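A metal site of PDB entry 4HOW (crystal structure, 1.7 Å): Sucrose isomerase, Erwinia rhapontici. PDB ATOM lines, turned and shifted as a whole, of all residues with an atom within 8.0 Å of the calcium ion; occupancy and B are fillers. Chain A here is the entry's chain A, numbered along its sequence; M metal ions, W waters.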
ATOM      1  N   PRO A  58      -1.713  16.086 -19.386  1.00  0.00           N
ATOM      2  CA  PRO A  58      -2.709  15.809 -18.318  1.00  0.00           C
ATOM      3  C   PRO A  58      -2.148  16.058 -16.914  1.00  0.00           C
ATOM      4  O   PRO A  58      -2.871  16.506 -16.111  1.00  0.00           O
ATOM      5  CB  PRO A  58      -3.092  14.348 -18.584  1.00  0.00           C
ATOM      6  CG  PRO A  58      -2.911  14.192 -20.121  1.00  0.00           C
ATOM      7  CD  PRO A  58      -1.615  15.022 -20.418  1.00  0.00           C
ATOM      8  N   ARG A  59      -0.883  15.761 -16.686  1.00  0.00           N
ATOM      9  CA  ARG A  59      -0.299  15.854 -15.343  1.00  0.00           C
ATOM     10  C   ARG A  59      -0.462  17.307 -14.793  1.00  0.00           C
ATOM     11  O   ARG A  59      -0.454  17.509 -13.583  1.00  0.00           O
ATOM     12  CB  ARG A  59       1.233  15.599 -15.511  1.00  0.00           C
ATOM     13  CG  ARG A  59       1.949  15.280 -14.190  1.00  0.00           C
ATOM     14  CD  ARG A  59       3.421  14.967 -14.545  1.00  0.00           C
ATOM     15  NE  ARG A  59       4.138  14.812 -13.283  1.00  0.00           N
ATOM     16  CZ  ARG A  59       4.127  13.738 -12.489  1.00  0.00           C
ATOM     17  NH1 ARG A  59       3.548  12.541 -12.826  1.00  0.00           N
ATOM     18  NH2 ARG A  59       4.825  13.821 -11.347  1.00  0.00           N
ATOM     19  N   LYS A  62      -5.696  19.705 -14.920  1.00  0.00           N
ATOM     20  CA  LYS A  62      -6.613  19.949 -13.803  1.00  0.00           C
ATOM     21  C   LYS A  62      -6.709  18.695 -12.921  1.00  0.00           C
ATOM     22  O   LYS A  62      -6.996  17.614 -13.408  1.00  0.00           O
ATOM     23  CB  LYS A  62      -8.012  20.345 -14.321  1.00  0.00           C
ATOM     24  CG  LYS A  62      -9.053  20.379 -13.225  1.00  0.00           C
ATOM     25  CD  LYS A  62      -8.620  21.323 -12.114  1.00  0.00           C
ATOM     26  CE  LYS A  62      -9.735  21.420 -11.054  1.00  0.00           C
ATOM     27  NZ  LYS A  62     -10.966  22.086 -11.573  1.00  0.00           N
ATOM     28  N   ASP A  63      -6.441  18.890 -11.602  1.00  0.00           N
ATOM     29  CA  ASP A  63      -6.478  17.789 -10.587  1.00  0.00           C
ATOM     30  C   ASP A  63      -7.885  17.846  -9.977  1.00  0.00           C
ATOM     31  O   ASP A  63      -8.335  18.908  -9.477  1.00  0.00           O
ATOM     32  CB  ASP A  63      -5.398  18.130  -9.557  1.00  0.00           C
ATOM     33  CG  ASP A  63      -5.453  17.199  -8.339  1.00  0.00           C
ATOM     34  OD1 ASP A  63      -6.133  16.169  -8.460  1.00  0.00           O
ATOM     35  OD2 ASP A  63      -4.827  17.531  -7.301  1.00  0.00           O
ATOM     36  N   THR A  64      -8.562  16.685  -9.985  1.00  0.00           N
ATOM     37  CA  THR A  64      -9.941  16.632  -9.475  1.00  0.00           C
ATOM     38  C   THR A  64      -9.977  15.789  -8.221  1.00  0.00           C
ATOM     39  O   THR A  64     -11.046  15.601  -7.728  1.00  0.00           O
ATOM     40  CB  THR A  64     -10.955  16.117 -10.509  1.00  0.00           C
ATOM     41  OG1 THR A  64     -10.566  14.791 -10.975  1.00  0.00           O
ATOM     42  CG2 THR A  64     -11.109  17.158 -11.719  1.00  0.00           C
ATOM     43  N   ASN A  65      -8.871  15.304  -7.713  1.00  0.00           N
ATOM     44  CA  ASN A  65      -8.969  14.515  -6.435  1.00  0.00           C
ATOM     45  C   ASN A  65      -7.986  14.902  -5.342  1.00  0.00           C
ATOM     46  O   ASN A  65      -7.784  14.140  -4.391  1.00  0.00           O
ATOM     47  CB  ASN A  65      -8.877  13.018  -6.730  1.00  0.00           C
ATOM     48  CG  ASN A  65      -7.658  12.672  -7.525  1.00  0.00           C
ATOM     49  OD1 ASN A  65      -6.573  13.264  -7.356  1.00  0.00           O
ATOM     50  ND2 ASN A  65      -7.827  11.747  -8.479  1.00  0.00           N
ATOM     51  N   GLY A  66      -7.278  16.007  -5.532  1.00  0.00           N
ATOM     52  CA  GLY A  66      -6.454  16.609  -4.493  1.00  0.00           C
ATOM     53  C   GLY A  66      -5.102  15.961  -4.319  1.00  0.00           C
ATOM     54  O   GLY A  66      -4.426  16.333  -3.359  1.00  0.00           O
ATOM     55  N   ASP A  67      -4.654  15.039  -5.213  1.00  0.00           N
ATOM     56  CA  ASP A  67      -3.293  14.499  -5.092  1.00  0.00           C
ATOM     57  C   ASP A  67      -2.135  15.349  -5.678  1.00  0.00           C
ATOM     58  O   ASP A  67      -0.948  14.985  -5.580  1.00  0.00           O
ATOM     59  CB  ASP A  67      -3.200  13.034  -5.569  1.00  0.00           C
ATOM     60  CG  ASP A  67      -3.418  12.900  -7.039  1.00  0.00           C
ATOM     61  OD1 ASP A  67      -3.707  13.973  -7.681  1.00  0.00           O
ATOM     62  OD2 ASP A  67      -3.330  11.744  -7.563  1.00  0.00           O
ATOM     63  N   GLY A  68      -2.531  16.483  -6.245  1.00  0.00           N
ATOM     64  CA  GLY A  68      -1.556  17.386  -6.800  1.00  0.00           C
ATOM     65  C   GLY A  68      -1.260  17.144  -8.301  1.00  0.00           C
ATOM     66  O   GLY A  68      -0.410  17.844  -8.871  1.00  0.00           O
ATOM     67  N   ILE A  69      -1.834  16.069  -8.835  1.00  0.00           N
ATOM     68  CA  ILE A  69      -1.509  15.582 -10.209  1.00  0.00           C
ATOM     69  C   ILE A  69      -2.757  15.748 -11.051  1.00  0.00           C
ATOM     70  O   ILE A  69      -3.860  15.339 -10.668  1.00  0.00           O
ATOM     71  CB  ILE A  69      -0.937  14.160 -10.194  1.00  0.00           C
ATOM     72  CG1 ILE A  69       0.462  14.231  -9.551  1.00  0.00           C
ATOM     73  CG2 ILE A  69      -0.753  13.648 -11.659  1.00  0.00           C
ATOM     74  CD1 ILE A  69       1.086  12.869  -9.272  1.00  0.00           C
ATOM     75  N   GLY A  70      -2.665  16.377 -12.227  1.00  0.00           N
ATOM     76  CA  GLY A  70      -3.890  16.483 -13.026  1.00  0.00           C
ATOM     77  C   GLY A  70      -4.312  15.076 -13.552  1.00  0.00           C
ATOM     78  O   GLY A  70      -3.524  14.127 -13.640  1.00  0.00           O
ATOM     79  N   ASP A  71      -5.571  14.990 -13.927  1.00  0.00           N
ATOM     80  CA  ASP A  71      -6.087  13.642 -14.327  1.00  0.00           C
ATOM     81  C   ASP A  71      -7.174  13.734 -15.366  1.00  0.00           C
ATOM     82  O   ASP A  71      -7.565  14.844 -15.808  1.00  0.00           O
ATOM     83  CB  ASP A  71      -6.725  12.988 -13.052  1.00  0.00           C
ATOM     84  CG  ASP A  71      -7.635  13.962 -12.244  1.00  0.00           C
ATOM     85  OD1 ASP A  71      -8.717  14.393 -12.716  1.00  0.00           O
ATOM     86  OD2 ASP A  71      -7.298  14.364 -11.046  1.00  0.00           O
ATOM     87  N   LEU A  72      -7.642  12.579 -15.873  1.00  0.00           N
ATOM     88  CA  LEU A  72      -8.608  12.636 -17.002  1.00  0.00           C
ATOM     89  C   LEU A  72      -9.914  13.293 -16.692  1.00  0.00           C
ATOM     90  O   LEU A  72     -10.494  14.026 -17.511  1.00  0.00           O
ATOM     91  CB  LEU A  72      -8.840  11.163 -17.544  1.00  0.00           C
ATOM     92  CG  LEU A  72      -7.651  10.474 -18.156  1.00  0.00           C
ATOM     93  CD1 LEU A  72      -8.067   9.015 -18.491  1.00  0.00           C
ATOM     94  CD2 LEU A  72      -7.214  11.114 -19.445  1.00  0.00           C
ATOM     95  N   ASN A  73     -10.470  13.047 -15.500  1.00  0.00           N
ATOM     96  CA  ASN A  73     -11.659  13.762 -15.140  1.00  0.00           C
ATOM     97  C   ASN A  73     -11.470  15.285 -15.187  1.00  0.00           C
ATOM     98  O   ASN A  73     -12.410  16.024 -15.503  1.00  0.00           O
ATOM     99  CB  ASN A  73     -12.074  13.339 -13.734  1.00  0.00           C
ATOM    100  CG  ASN A  73     -12.746  11.949 -13.747  1.00  0.00           C
ATOM    101  OD1 ASN A  73     -13.122  11.434 -14.810  1.00  0.00           O
ATOM    102  ND2 ASN A  73     -12.838  11.320 -12.571  1.00  0.00           N
ATOM    103  N   GLY A  74     -10.262  15.743 -14.892  1.00  0.00           N
ATOM    104  CA  GLY A  74      -9.945  17.155 -14.935  1.00  0.00           C
ATOM    105  C   GLY A  74     -10.006  17.678 -16.389  1.00  0.00           C
ATOM    106  O   GLY A  74     -10.431  18.825 -16.610  1.00  0.00           O
ATOM    107  N   LYS A 115      -2.248   5.332 -13.413  1.00  0.00           N
ATOM    108  CA  LYS A 115      -3.016   5.291 -12.172  1.00  0.00           C
ATOM    109  C   LYS A 115      -3.426   6.670 -11.678  1.00  0.00           C
ATOM    110  O   LYS A 115      -4.606   6.907 -11.333  1.00  0.00           O
ATOM    111  CB  LYS A 115      -2.078   4.631 -11.114  1.00  0.00           C
ATOM    112  CG  LYS A 115      -2.762   4.427  -9.760  1.00  0.00           C
ATOM    113  CD  LYS A 115      -1.798   3.724  -8.773  1.00  0.00           C
ATOM    114  CE  LYS A 115      -0.672   4.633  -8.261  1.00  0.00           C
ATOM    115  NZ  LYS A 115      -0.328   4.110  -6.911  1.00  0.00           N
ATOM    116  N   GLU A 116      -2.471   7.618 -11.782  1.00  0.00           N
ATOM    117  CA  GLU A 116      -2.738   9.010 -11.388  1.00  0.00           C
ATOM    118  C   GLU A 116      -3.755   9.704 -12.273  1.00  0.00           C
ATOM    119  O   GLU A 116      -4.354  10.732 -11.886  1.00  0.00           O
ATOM    120  CB  GLU A 116      -1.431   9.800 -11.444  1.00  0.00           C
ATOM    121  CG  GLU A 116      -0.398   9.409 -10.359  1.00  0.00           C
ATOM    122  CD  GLU A 116       0.504   8.267 -10.694  1.00  0.00           C
ATOM    123  OE1 GLU A 116       0.390   7.648 -11.781  1.00  0.00           O
ATOM    124  OE2 GLU A 116       1.366   7.974  -9.853  1.00  0.00           O
ATOM    125  N   TYR A 117      -3.943   9.196 -13.487  1.00  0.00           N
ATOM    126  CA  TYR A 117      -4.905   9.854 -14.419  1.00  0.00           C
ATOM    127  C   TYR A 117      -6.320   9.314 -14.329  1.00  0.00           C
ATOM    128  O   TYR A 117      -7.272  10.011 -14.720  1.00  0.00           O
ATOM    129  CB  TYR A 117      -4.425   9.842 -15.887  1.00  0.00           C
ATOM    130  CG  TYR A 117      -3.117  10.562 -16.143  1.00  0.00           C
ATOM    131  CD1 TYR A 117      -2.536  11.449 -15.189  1.00  0.00           C
ATOM    132  CD2 TYR A 117      -2.492  10.386 -17.336  1.00  0.00           C
ATOM    133  CE1 TYR A 117      -1.281  12.050 -15.446  1.00  0.00           C
ATOM    134  CE2 TYR A 117      -1.262  11.049 -17.623  1.00  0.00           C
ATOM    135  CZ  TYR A 117      -0.732  11.902 -16.678  1.00  0.00           C
ATOM    136  OH  TYR A 117       0.481  12.477 -16.923  1.00  0.00           O
ATOM    137  N   GLY A 118      -6.476   8.093 -13.793  1.00  0.00           N
ATOM    138  CA  GLY A 118      -7.860   7.640 -13.601  1.00  0.00           C
ATOM    139  C   GLY A 118      -7.980   6.199 -14.141  1.00  0.00           C
ATOM    140  O   GLY A 118      -7.018   5.432 -14.027  1.00  0.00           O
ATOM    141  N   PHE A 473      -6.052  24.910  -9.559  1.00  0.00           N
ATOM    142  CA  PHE A 473      -5.592  23.715 -10.259  1.00  0.00           C
ATOM    143  C   PHE A 473      -5.855  22.494  -9.321  1.00  0.00           C
ATOM    144  O   PHE A 473      -6.107  21.351  -9.777  1.00  0.00           O
ATOM    145  CB  PHE A 473      -4.100  23.824 -10.512  1.00  0.00           C
ATOM    146  CG  PHE A 473      -3.452  22.505 -10.870  1.00  0.00           C
ATOM    147  CD1 PHE A 473      -3.688  21.880 -12.135  1.00  0.00           C
ATOM    148  CD2 PHE A 473      -2.650  21.837  -9.955  1.00  0.00           C
ATOM    149  CE1 PHE A 473      -3.087  20.635 -12.413  1.00  0.00           C
ATOM    150  CE2 PHE A 473      -2.043  20.608 -10.285  1.00  0.00           C
ATOM    151  CZ  PHE A 473      -2.261  19.977 -11.525  1.00  0.00           C
ATOM    152  N   THR A 474      -5.629  22.663  -8.004  1.00  0.00           N
ATOM    153  CA  THR A 474      -5.724  21.466  -7.114  1.00  0.00           C
ATOM    154  C   THR A 474      -6.242  21.977  -5.722  1.00  0.00           C
ATOM    155  O   THR A 474      -5.998  23.147  -5.363  1.00  0.00           O
ATOM    156  CB  THR A 474      -4.350  20.795  -6.878  1.00  0.00           C
ATOM    157  OG1 THR A 474      -4.471  19.617  -6.029  1.00  0.00           O
ATOM    158  CG2 THR A 474      -3.221  21.737  -6.311  1.00  0.00           C
HETATM  159 CA    CA M   1      -5.430  14.180  -9.467  1.00  0.00          CA
HETATM  160  O   HOH W   1      -4.937  11.770  -9.704  1.00  0.00           O
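Water W1 lies within hydrogen-bond range of O of Glu 116 (2.5 Å), OD2 of Asp 67 (2.7 Å) and ND2 of Asn 65 (3.1 Å).
Within 4 Å of the calcium ion: Asp 63, Asn 65, Asp 67, Ile 69 and Asp 71.
The calcium ion is bound by O of Ile 69, OD1 of Asp 63, OD2 of Asp 71, water W1, OD1 of Asp 67 and OD1 of Asn 65.
OG1 of Thr 474 lies within hydrogen-bond range of OD2 of Asp 63, at 2.5 Å. The backbone NH (N) of Gly 66 lies close to the side-chain carboxylate (OD2) of Asp 63, 3.4 Å away. N of Asp 71 is in hydrogen-bond range of O of Lys 62 (3.0 Å). The side-chain carboxylate (OD2) of Asp 63 lies within hydrogen-bond range of the backbone NH (N) of Gly 68 (2.7 Å). OD1 of Asp 71 sits at hydrogen-bond distance from OG1 of Thr 64 (2.6 Å). The backbone NH of Asp 63 is in hydrogen-bond range of the backbone carbonyl oxygen of Phe 473, at 3.1 Å. OD1 of Asp 71 is in hydrogen-bond range of N of Gly 74, at 3.0 Å.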
